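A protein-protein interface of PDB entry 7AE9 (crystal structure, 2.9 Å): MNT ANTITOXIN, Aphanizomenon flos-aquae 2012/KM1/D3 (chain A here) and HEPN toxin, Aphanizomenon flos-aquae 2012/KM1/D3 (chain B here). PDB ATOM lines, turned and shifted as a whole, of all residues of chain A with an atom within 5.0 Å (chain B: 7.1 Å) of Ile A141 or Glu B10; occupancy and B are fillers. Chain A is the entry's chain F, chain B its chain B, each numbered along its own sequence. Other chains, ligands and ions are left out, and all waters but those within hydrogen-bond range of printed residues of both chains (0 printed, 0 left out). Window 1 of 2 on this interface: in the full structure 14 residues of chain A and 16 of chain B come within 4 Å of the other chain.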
ATOM      1  N   GLU A 134     -10.932  32.020 -22.824  1.00  0.00           N
ATOM      2  CA  GLU A 134     -10.349  31.665 -24.113  1.00  0.00           C
ATOM      3  C   GLU A 134      -9.506  32.799 -24.691  1.00  0.00           C
ATOM      4  O   GLU A 134      -8.506  32.538 -25.369  1.00  0.00           O
ATOM      5  CB  GLU A 134     -11.429  31.152 -25.076  1.00  0.00           C
ATOM      6  CG  GLU A 134     -12.462  32.078 -25.611  1.00  0.00           C
ATOM      7  CD  GLU A 134     -13.494  31.302 -26.429  1.00  0.00           C
ATOM      8  OE1 GLU A 134     -14.192  30.441 -25.847  1.00  0.00           O
ATOM      9  OE2 GLU A 134     -13.580  31.520 -27.657  1.00  0.00           O
ATOM     10  N   LYS A 137      -6.093  32.466 -22.994  1.00  0.00           N
ATOM     11  CA  LYS A 137      -5.286  31.365 -23.497  1.00  0.00           C
ATOM     12  C   LYS A 137      -4.711  31.684 -24.879  1.00  0.00           C
ATOM     13  O   LYS A 137      -3.572  31.309 -25.188  1.00  0.00           O
ATOM     14  CB  LYS A 137      -6.113  30.080 -23.501  1.00  0.00           C
ATOM     15  CG  LYS A 137      -6.439  29.572 -22.105  1.00  0.00           C
ATOM     16  CD  LYS A 137      -6.970  28.137 -22.146  1.00  0.00           C
ATOM     17  CE  LYS A 137      -7.138  27.551 -20.748  1.00  0.00           C
ATOM     18  NZ  LYS A 137      -6.083  28.051 -19.812  1.00  0.00           N
ATOM     19  N   LEU A 138      -5.488  32.355 -25.732  1.00  0.00           N
ATOM     20  CA  LEU A 138      -4.946  32.754 -27.026  1.00  0.00           C
ATOM     21  C   LEU A 138      -3.744  33.677 -26.866  1.00  0.00           C
ATOM     22  O   LEU A 138      -2.840  33.669 -27.705  1.00  0.00           O
ATOM     23  CB  LEU A 138      -6.027  33.424 -27.876  1.00  0.00           C
ATOM     24  CG  LEU A 138      -7.066  32.451 -28.443  1.00  0.00           C
ATOM     25  CD1 LEU A 138      -8.214  33.171 -29.139  1.00  0.00           C
ATOM     26  CD2 LEU A 138      -6.406  31.436 -29.368  1.00  0.00           C
ATOM     27  N   GLU A 139      -3.715  34.478 -25.804  1.00  0.00           N
ATOM     28  CA  GLU A 139      -2.558  35.333 -25.558  1.00  0.00           C
ATOM     29  C   GLU A 139      -1.327  34.508 -25.200  1.00  0.00           C
ATOM     30  O   GLU A 139      -0.217  34.843 -25.619  1.00  0.00           O
ATOM     31  CB  GLU A 139      -2.881  36.349 -24.458  1.00  0.00           C
ATOM     32  CG  GLU A 139      -1.983  37.591 -24.395  1.00  0.00           C
ATOM     33  CD  GLU A 139      -0.546  37.290 -23.988  1.00  0.00           C
ATOM     34  OE1 GLU A 139       0.370  37.722 -24.717  1.00  0.00           O
ATOM     35  OE2 GLU A 139      -0.325  36.614 -22.957  1.00  0.00           O
ATOM     36  N   ASN A 140      -1.495  33.420 -24.438  1.00  0.00           N
ATOM     37  CA  ASN A 140      -0.341  32.575 -24.123  1.00  0.00           C
ATOM     38  C   ASN A 140       0.144  31.812 -25.341  1.00  0.00           C
ATOM     39  O   ASN A 140       1.350  31.604 -25.503  1.00  0.00           O
ATOM     40  CB  ASN A 140      -0.681  31.578 -23.015  1.00  0.00           C
ATOM     41  CG  ASN A 140      -0.727  32.218 -21.649  1.00  0.00           C
ATOM     42  OD1 ASN A 140       0.042  33.133 -21.348  1.00  0.00           O
ATOM     43  ND2 ASN A 140      -1.662  31.764 -20.820  1.00  0.00           N
ATOM     44  N   ILE A 141      -0.781  31.410 -26.208  1.00  0.00           N
ATOM     45  CA  ILE A 141      -0.426  30.691 -27.423  1.00  0.00           C
ATOM     46  C   ILE A 141       0.323  31.603 -28.380  1.00  0.00           C
ATOM     47  O   ILE A 141       1.318  31.202 -28.995  1.00  0.00           O
ATOM     48  CB  ILE A 141      -1.699  30.117 -28.062  1.00  0.00           C
ATOM     49  CG1 ILE A 141      -2.313  29.073 -27.130  1.00  0.00           C
ATOM     50  CG2 ILE A 141      -1.402  29.550 -29.459  1.00  0.00           C
ATOM     51  CD1 ILE A 141      -3.724  28.711 -27.494  1.00  0.00           C
ATOM     52  N   GLU A 142      -0.153  32.842 -28.538  1.00  0.00           N
ATOM     53  CA  GLU A 142       0.514  33.771 -29.438  1.00  0.00           C
ATOM     54  C   GLU A 142       1.887  34.182 -28.917  1.00  0.00           C
ATOM     55  O   GLU A 142       2.802  34.427 -29.712  1.00  0.00           O
ATOM     56  CB  GLU A 142      -0.362  35.000 -29.680  1.00  0.00           C
ATOM     57  CG  GLU A 142       0.227  35.902 -30.739  1.00  0.00           C
ATOM     58  CD  GLU A 142       0.274  35.240 -32.113  1.00  0.00           C
ATOM     59  OE1 GLU A 142      -0.683  34.512 -32.462  1.00  0.00           O
ATOM     60  OE2 GLU A 142       1.293  35.416 -32.822  1.00  0.00           O
ATOM     61  N   ASN A 143       2.052  34.275 -27.599  1.00  0.00           N
ATOM     62  CA  ASN A 143       3.366  34.577 -27.050  1.00  0.00           C
ATOM     63  C   ASN A 143       4.320  33.423 -27.298  1.00  0.00           C
ATOM     64  O   ASN A 143       5.510  33.637 -27.554  1.00  0.00           O
ATOM     65  CB  ASN A 143       3.255  34.883 -25.560  1.00  0.00           C
ATOM     66  CG  ASN A 143       4.601  35.005 -24.891  1.00  0.00           C
ATOM     67  OD1 ASN A 143       4.999  34.131 -24.116  1.00  0.00           O
ATOM     68  ND2 ASN A 143       5.322  36.081 -25.194  1.00  0.00           N
ATOM     69  N   PHE A 144       3.814  32.189 -27.217  1.00  0.00           N
ATOM     70  CA  PHE A 144       4.637  31.035 -27.536  1.00  0.00           C
ATOM     71  C   PHE A 144       5.092  31.106 -28.976  1.00  0.00           C
ATOM     72  O   PHE A 144       6.284  30.973 -29.271  1.00  0.00           O
ATOM     73  CB  PHE A 144       3.859  29.739 -27.294  1.00  0.00           C
ATOM     74  CG  PHE A 144       4.510  28.522 -27.912  1.00  0.00           C
ATOM     75  CD1 PHE A 144       5.486  27.818 -27.224  1.00  0.00           C
ATOM     76  CD2 PHE A 144       4.161  28.100 -29.191  1.00  0.00           C
ATOM     77  CE1 PHE A 144       6.110  26.717 -27.795  1.00  0.00           C
ATOM     78  CE2 PHE A 144       4.767  27.006 -29.764  1.00  0.00           C
ATOM     79  CZ  PHE A 144       5.752  26.308 -29.065  1.00  0.00           C
ATOM     80  N   LEU A 145       4.145  31.334 -29.887  1.00  0.00           N
ATOM     81  CA  LEU A 145       4.471  31.386 -31.302  1.00  0.00           C
ATOM     82  C   LEU A 145       5.448  32.510 -31.588  1.00  0.00           C
ATOM     83  O   LEU A 145       6.325  32.381 -32.447  1.00  0.00           O
ATOM     84  CB  LEU A 145       3.194  31.552 -32.109  1.00  0.00           C
ATOM     85  CG  LEU A 145       2.216  30.382 -32.096  1.00  0.00           C
ATOM     86  CD1 LEU A 145       0.894  30.772 -32.749  1.00  0.00           C
ATOM     87  CD2 LEU A 145       2.809  29.201 -32.819  1.00  0.00           C
ATOM     88  N   GLU B   5     -15.652  23.618 -29.736  1.00  0.00           N
ATOM     89  CA  GLU B   5     -15.329  24.333 -28.507  1.00  0.00           C
ATOM     90  C   GLU B   5     -13.920  24.915 -28.544  1.00  0.00           C
ATOM     91  O   GLU B   5     -12.964  24.218 -28.175  1.00  0.00           O
ATOM     92  CB  GLU B   5     -15.455  23.366 -27.329  1.00  0.00           C
ATOM     93  CG  GLU B   5     -16.785  22.669 -27.160  1.00  0.00           C
ATOM     94  CD  GLU B   5     -17.791  23.518 -26.460  1.00  0.00           C
ATOM     95  OE1 GLU B   5     -17.413  24.619 -26.006  1.00  0.00           O
ATOM     96  OE2 GLU B   5     -18.950  23.075 -26.338  1.00  0.00           O
ATOM     97  N   PRO B   6     -13.732  26.186 -28.918  1.00  0.00           N
ATOM     98  CA  PRO B   6     -12.363  26.738 -28.920  1.00  0.00           C
ATOM     99  C   PRO B   6     -11.644  26.632 -27.581  1.00  0.00           C
ATOM    100  O   PRO B   6     -10.426  26.415 -27.557  1.00  0.00           O
ATOM    101  CB  PRO B   6     -12.576  28.195 -29.359  1.00  0.00           C
ATOM    102  CG  PRO B   6     -13.803  28.138 -30.188  1.00  0.00           C
ATOM    103  CD  PRO B   6     -14.690  27.111 -29.542  1.00  0.00           C
ATOM    104  N   VAL B   7     -12.356  26.762 -26.463  1.00  0.00           N
ATOM    105  CA  VAL B   7     -11.665  26.727 -25.178  1.00  0.00           C
ATOM    106  C   VAL B   7     -11.055  25.351 -24.941  1.00  0.00           C
ATOM    107  O   VAL B   7     -10.007  25.231 -24.300  1.00  0.00           O
ATOM    108  CB  VAL B   7     -12.615  27.133 -24.038  1.00  0.00           C
ATOM    109  CG1 VAL B   7     -13.752  26.125 -23.879  1.00  0.00           C
ATOM    110  CG2 VAL B   7     -11.847  27.311 -22.762  1.00  0.00           C
ATOM    111  N   ILE B   8     -11.669  24.299 -25.481  1.00  0.00           N
ATOM    112  CA  ILE B   8     -11.116  22.960 -25.331  1.00  0.00           C
ATOM    113  C   ILE B   8      -9.811  22.824 -26.112  1.00  0.00           C
ATOM    114  O   ILE B   8      -8.789  22.368 -25.583  1.00  0.00           O
ATOM    115  CB  ILE B   8     -12.156  21.917 -25.773  1.00  0.00           C
ATOM    116  CG1 ILE B   8     -13.379  21.998 -24.867  1.00  0.00           C
ATOM    117  CG2 ILE B   8     -11.557  20.530 -25.776  1.00  0.00           C
ATOM    118  CD1 ILE B   8     -14.402  20.907 -25.114  1.00  0.00           C
ATOM    119  N   ILE B   9      -9.810  23.259 -27.369  1.00  0.00           N
ATOM    120  CA  ILE B   9      -8.596  23.154 -28.164  1.00  0.00           C
ATOM    121  C   ILE B   9      -7.514  24.068 -27.607  1.00  0.00           C
ATOM    122  O   ILE B   9      -6.338  23.693 -27.543  1.00  0.00           O
ATOM    123  CB  ILE B   9      -8.907  23.472 -29.631  1.00  0.00           C
ATOM    124  CG1 ILE B   9      -9.922  22.472 -30.173  1.00  0.00           C
ATOM    125  CG2 ILE B   9      -7.626  23.483 -30.462  1.00  0.00           C
ATOM    126  CD1 ILE B   9     -10.348  22.800 -31.559  1.00  0.00           C
ATOM    127  N   GLU B  10      -7.890  25.288 -27.215  1.00  0.00           N
ATOM    128  CA  GLU B  10      -6.907  26.244 -26.723  1.00  0.00           C
ATOM    129  C   GLU B  10      -6.261  25.789 -25.421  1.00  0.00           C
ATOM    130  O   GLU B  10      -5.106  26.135 -25.152  1.00  0.00           O
ATOM    131  CB  GLU B  10      -7.563  27.602 -26.538  1.00  0.00           C
ATOM    132  CG  GLU B  10      -7.862  28.311 -27.829  1.00  0.00           C
ATOM    133  CD  GLU B  10      -9.022  29.267 -27.699  1.00  0.00           C
ATOM    134  OE1 GLU B  10      -9.442  29.500 -26.556  1.00  0.00           O
ATOM    135  OE2 GLU B  10      -9.512  29.784 -28.728  1.00  0.00           O
ATOM    136  N   THR B  11      -6.971  25.025 -24.596  1.00  0.00           N
ATOM    137  CA  THR B  11      -6.342  24.557 -23.369  1.00  0.00           C
ATOM    138  C   THR B  11      -5.249  23.551 -23.673  1.00  0.00           C
ATOM    139  O   THR B  11      -4.145  23.632 -23.121  1.00  0.00           O
ATOM    140  CB  THR B  11      -7.376  23.942 -22.422  1.00  0.00           C
ATOM    141  OG1 THR B  11      -8.357  24.925 -22.053  1.00  0.00           O
ATOM    142  CG2 THR B  11      -6.696  23.379 -21.184  1.00  0.00           C
ATOM    143  N   ARG B  12      -5.536  22.610 -24.571  1.00  0.00           N
ATOM    144  CA  ARG B  12      -4.564  21.582 -24.914  1.00  0.00           C
ATOM    145  C   ARG B  12      -3.385  22.194 -25.664  1.00  0.00           C
ATOM    146  O   ARG B  12      -2.225  21.871 -25.386  1.00  0.00           O
ATOM    147  CB  ARG B  12      -5.269  20.510 -25.740  1.00  0.00           C
ATOM    148  CG  ARG B  12      -6.465  19.919 -24.981  1.00  0.00           C
ATOM    149  CD  ARG B  12      -6.078  18.941 -23.899  1.00  0.00           C
ATOM    150  NE  ARG B  12      -7.206  18.480 -23.077  1.00  0.00           N
ATOM    151  CZ  ARG B  12      -8.352  17.958 -23.520  1.00  0.00           C
ATOM    152  NH1 ARG B  12      -8.595  17.809 -24.813  1.00  0.00           N
ATOM    153  NH2 ARG B  12      -9.275  17.579 -22.649  1.00  0.00           N
ATOM    154  N   LEU B  13      -3.670  23.136 -26.565  1.00  0.00           N
ATOM    155  CA  LEU B  13      -2.622  23.852 -27.285  1.00  0.00           C
ATOM    156  C   LEU B  13      -1.721  24.625 -26.331  1.00  0.00           C
ATOM    157  O   LEU B  13      -0.504  24.706 -26.539  1.00  0.00           O
ATOM    158  CB  LEU B  13      -3.262  24.799 -28.292  1.00  0.00           C
ATOM    159  CG  LEU B  13      -2.512  24.984 -29.599  1.00  0.00           C
ATOM    160  CD1 LEU B  13      -2.295  23.644 -30.254  1.00  0.00           C
ATOM    161  CD2 LEU B  13      -3.328  25.874 -30.501  1.00  0.00           C
ATOM    162  N   GLU B  14      -2.304  25.216 -25.287  1.00  0.00           N
ATOM    163  CA  GLU B  14      -1.500  25.952 -24.317  1.00  0.00           C
ATOM    164  C   GLU B  14      -0.613  25.011 -23.505  1.00  0.00           C
ATOM    165  O   GLU B  14       0.502  25.378 -23.113  1.00  0.00           O
ATOM    166  CB  GLU B  14      -2.402  26.779 -23.405  1.00  0.00           C
ATOM    167  CG  GLU B  14      -1.640  27.852 -22.657  1.00  0.00           C
ATOM    168  CD  GLU B  14      -2.415  28.411 -21.492  1.00  0.00           C
ATOM    169  OE1 GLU B  14      -3.661  28.367 -21.521  1.00  0.00           O
ATOM    170  OE2 GLU B  14      -1.772  28.887 -20.535  1.00  0.00           O
ATOM    171  N   LEU B  15      -1.099  23.801 -23.210  1.00  0.00           N
ATOM    172  CA  LEU B  15      -0.244  22.829 -22.546  1.00  0.00           C
ATOM    173  C   LEU B  15       0.904  22.398 -23.456  1.00  0.00           C
ATOM    174  O   LEU B  15       2.060  22.328 -23.017  1.00  0.00           O
ATOM    175  CB  LEU B  15      -1.071  21.627 -22.090  1.00  0.00           C
ATOM    176  CG  LEU B  15      -1.924  21.859 -20.835  1.00  0.00           C
ATOM    177  CD1 LEU B  15      -2.754  20.630 -20.523  1.00  0.00           C
ATOM    178  CD2 LEU B  15      -1.069  22.272 -19.639  1.00  0.00           C
ATOM    179  N   ILE B  16       0.607  22.121 -24.731  1.00  0.00           N
ATOM    180  CA  ILE B  16       1.655  21.739 -25.674  1.00  0.00           C
ATOM    181  C   ILE B  16       2.769  22.771 -25.678  1.00  0.00           C
ATOM    182  O   ILE B  16       3.956  22.427 -25.641  1.00  0.00           O
ATOM    183  CB  ILE B  16       1.066  21.550 -27.078  1.00  0.00           C
ATOM    184  CG1 ILE B  16       0.209  20.296 -27.115  1.00  0.00           C
ATOM    185  CG2 ILE B  16       2.178  21.447 -28.086  1.00  0.00           C
ATOM    186  CD1 ILE B  16      -0.408  20.020 -28.453  1.00  0.00           C
ATOM    187  N   GLY B  17       2.407  24.054 -25.697  1.00  0.00           N
ATOM    188  CA  GLY B  17       3.423  25.089 -25.661  1.00  0.00           C
ATOM    189  C   GLY B  17       4.240  25.053 -24.385  1.00  0.00           C
ATOM    190  O   GLY B  17       5.449  25.293 -24.406  1.00  0.00           O
ATOM    191  N   ILE B  58      -6.703  17.155 -29.233  1.00  0.00           N
ATOM    192  CA  ILE B  58      -7.151  18.201 -30.138  1.00  0.00           C
ATOM    193  C   ILE B  58      -7.704  17.586 -31.414  1.00  0.00           C
ATOM    194  O   ILE B  58      -8.811  17.915 -31.850  1.00  0.00           O
ATOM    195  CB  ILE B  58      -5.998  19.165 -30.440  1.00  0.00           C
ATOM    196  CG1 ILE B  58      -5.676  19.980 -29.203  1.00  0.00           C
ATOM    197  CG2 ILE B  58      -6.353  20.070 -31.594  1.00  0.00           C
ATOM    198  CD1 ILE B  58      -4.486  20.867 -29.384  1.00  0.00           C
ATOM    199  N   VAL B 132       1.323  23.894 -33.485  1.00  0.00           N
ATOM    200  CA  VAL B 132       0.719  24.967 -32.698  1.00  0.00           C
ATOM    201  C   VAL B 132       0.308  26.109 -33.613  1.00  0.00           C
ATOM    202  O   VAL B 132      -0.831  26.582 -33.569  1.00  0.00           O
ATOM    203  CB  VAL B 132       1.675  25.454 -31.591  1.00  0.00           C
ATOM    204  CG1 VAL B 132       1.095  26.666 -30.894  1.00  0.00           C
ATOM    205  CG2 VAL B 132       1.938  24.363 -30.574  1.00  0.00           C
ATOM    206  N   ARG B 133       1.214  26.532 -34.493  1.00  0.00           N
ATOM    207  CA  ARG B 133       0.890  27.608 -35.426  1.00  0.00           C
ATOM    208  C   ARG B 133      -0.317  27.251 -36.286  1.00  0.00           C
ATOM    209  O   ARG B 133      -1.259  28.037 -36.416  1.00  0.00           O
ATOM    210  CB  ARG B 133       2.098  27.921 -36.301  1.00  0.00           C
ATOM    211  CG  ARG B 133       1.798  28.698 -37.545  1.00  0.00           C
ATOM    212  CD  ARG B 133       1.337  30.061 -37.237  1.00  0.00           C
ATOM    213  NE  ARG B 133       2.407  30.895 -36.707  1.00  0.00           N
ATOM    214  CZ  ARG B 133       2.185  32.104 -36.196  1.00  0.00           C
ATOM    215  NH1 ARG B 133       0.929  32.569 -36.161  1.00  0.00           N
ATOM    216  NH2 ARG B 133       3.196  32.833 -35.715  1.00  0.00           N
ATOM    217  N   ILE B 135      -2.762  24.948 -35.917  1.00  0.00           N
ATOM    218  CA  ILE B 135      -4.027  24.833 -35.192  1.00  0.00           C
ATOM    219  C   ILE B 135      -4.488  26.202 -34.713  1.00  0.00           C
ATOM    220  O   ILE B 135      -5.684  26.516 -34.749  1.00  0.00           O
ATOM    221  CB  ILE B 135      -3.904  23.838 -34.026  1.00  0.00           C
ATOM    222  CG1 ILE B 135      -3.534  22.443 -34.551  1.00  0.00           C
ATOM    223  CG2 ILE B 135      -5.213  23.764 -33.249  1.00  0.00           C
ATOM    224  CD1 ILE B 135      -4.617  21.778 -35.376  1.00  0.00           C
ATOM    225  N   ASN B 136      -3.545  27.050 -34.289  1.00  0.00           N
ATOM    226  CA  ASN B 136      -3.903  28.400 -33.864  1.00  0.00           C
ATOM    227  C   ASN B 136      -4.547  29.186 -34.996  1.00  0.00           C
ATOM    228  O   ASN B 136      -5.484  29.959 -34.778  1.00  0.00           O
ATOM    229  CB  ASN B 136      -2.680  29.144 -33.341  1.00  0.00           C
ATOM    230  CG  ASN B 136      -3.016  30.552 -32.920  1.00  0.00           C
ATOM    231  OD1 ASN B 136      -3.601  30.770 -31.862  1.00  0.00           O
ATOM    232  ND2 ASN B 136      -2.646  31.515 -33.737  1.00  0.00           N
ATOM    233  N   LEU B 139      -8.129  28.210 -35.286  1.00  0.00           N
ATOM    234  CA  LEU B 139      -8.955  28.824 -34.252  1.00  0.00           C
ATOM    235  C   LEU B 139      -9.325  30.251 -34.623  1.00  0.00           C
ATOM    236  O   LEU B 139     -10.488  30.644 -34.499  1.00  0.00           O
ATOM    237  CB  LEU B 139      -8.209  28.784 -32.918  1.00  0.00           C
ATOM    238  CG  LEU B 139      -8.224  27.424 -32.223  1.00  0.00           C
ATOM    239  CD1 LEU B 139      -7.377  27.456 -30.993  1.00  0.00           C
ATOM    240  CD2 LEU B 139      -9.649  27.046 -31.847  1.00  0.00           C
ATOM    241  N   ILE B 140      -8.353  31.034 -35.097  1.00  0.00           N
ATOM    242  CA  ILE B 140      -8.645  32.394 -35.539  1.00  0.00           C
ATOM    243  C   ILE B 140      -9.646  32.391 -36.686  1.00  0.00           C
ATOM    244  O   ILE B 140     -10.497  33.282 -36.773  1.00  0.00           O
ATOM    245  CB  ILE B 140      -7.337  33.124 -35.902  1.00  0.00           C
ATOM    246  CG1 ILE B 140      -6.604  33.548 -34.625  1.00  0.00           C
ATOM    247  CG2 ILE B 140      -7.606  34.327 -36.775  1.00  0.00           C
ATOM    248  CD1 ILE B 140      -5.187  34.038 -34.864  1.00  0.00           C
ATOM    249  N   GLU B 143     -13.222  32.342 -35.324  1.00  0.00           N
ATOM    250  CA  GLU B 143     -13.780  33.574 -34.773  1.00  0.00           C
ATOM    251  C   GLU B 143     -14.652  34.295 -35.795  1.00  0.00           C
ATOM    252  O   GLU B 143     -15.656  34.919 -35.429  1.00  0.00           O
ATOM    253  CB  GLU B 143     -12.658  34.494 -34.297  1.00  0.00           C
ATOM    254  CG  GLU B 143     -11.843  33.941 -33.141  1.00  0.00           C
ATOM    255  CD  GLU B 143     -10.766  34.904 -32.680  1.00  0.00           C
ATOM    256  OE1 GLU B 143     -10.326  35.743 -33.497  1.00  0.00           O
ATOM    257  OE2 GLU B 143     -10.365  34.832 -31.499  1.00  0.00           O
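Among the printed residues, merely in contact across the chains: Lys A137 with Thr B11 (3.2 Å), Ile A141 with Asn B136 (3.5 Å), Leu A145 with Arg B133 (3.5 Å), Leu A138 with Glu B10 (3.6 Å), Leu A138 with Glu B143 (3.6 Å), Leu A145 with Val B132 (3.6 Å), Phe A144 with Gly B17 (3.7 Å), Ile A141 with Glu B10 (3.7 Å), Leu A145 with Asn B136 (3.7 Å), Phe A144 with Val B132 (3.8 Å), Glu A142 with Asn B136 (3.8 Å), Leu A138 with Asn B136 (3.8 Å) and Glu A134 with Pro B6 (3.9 Å).
O of Val B7 lies within hydrogen-bond range of OG1 of Thr B11 (2.8 Å).
O of Glu A134 lies close to OE1 of Glu B10 (3.4 Å). The side-chain amino group (NZ) of Lys A137 is in salt-bridge range of the side-chain carboxylate (OE1) of Glu B14. ND2 of Asn A140 lies within hydrogen-bond range of OE2 of Glu B14 (2.9 Å).
Printed residues of chain B that touch a printed residue of chain A: Pro B6, Glu B10, Thr B11, Glu B14, Gly B17, Val B132, Arg B133, Asn B136 and Glu B143. Along chain B the printed residues that touch a printed residue of chain A span positions 6 to 143. Of the 10 printed residues of chain A, 8 touch a printed residue of chain B. Along chain A the printed residues that touch a printed residue of chain B span positions 134 to 145. Among the printed residues, Asp or Glu carboxylates within 4 Å of a Lys or Arg side-chain nitrogen of the other chain: Lys A137 with Glu B14 (3.0 Å).
Printed residues of chain B within 4 Å of Ile A141: Glu B10 (3.7 Å) and Asn B136 (3.5 Å). Of chain A, only Glu A134, Leu A138 and Ile A141 come within 4 Å of Glu B10. Printed residues of chain A within 4 Å of Glu B143: Leu A138 (3.6 Å). Of the printed residues of chain B, Asn A140 touches Glu B14. Ile B58 touches none of the printed residues of chain A.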
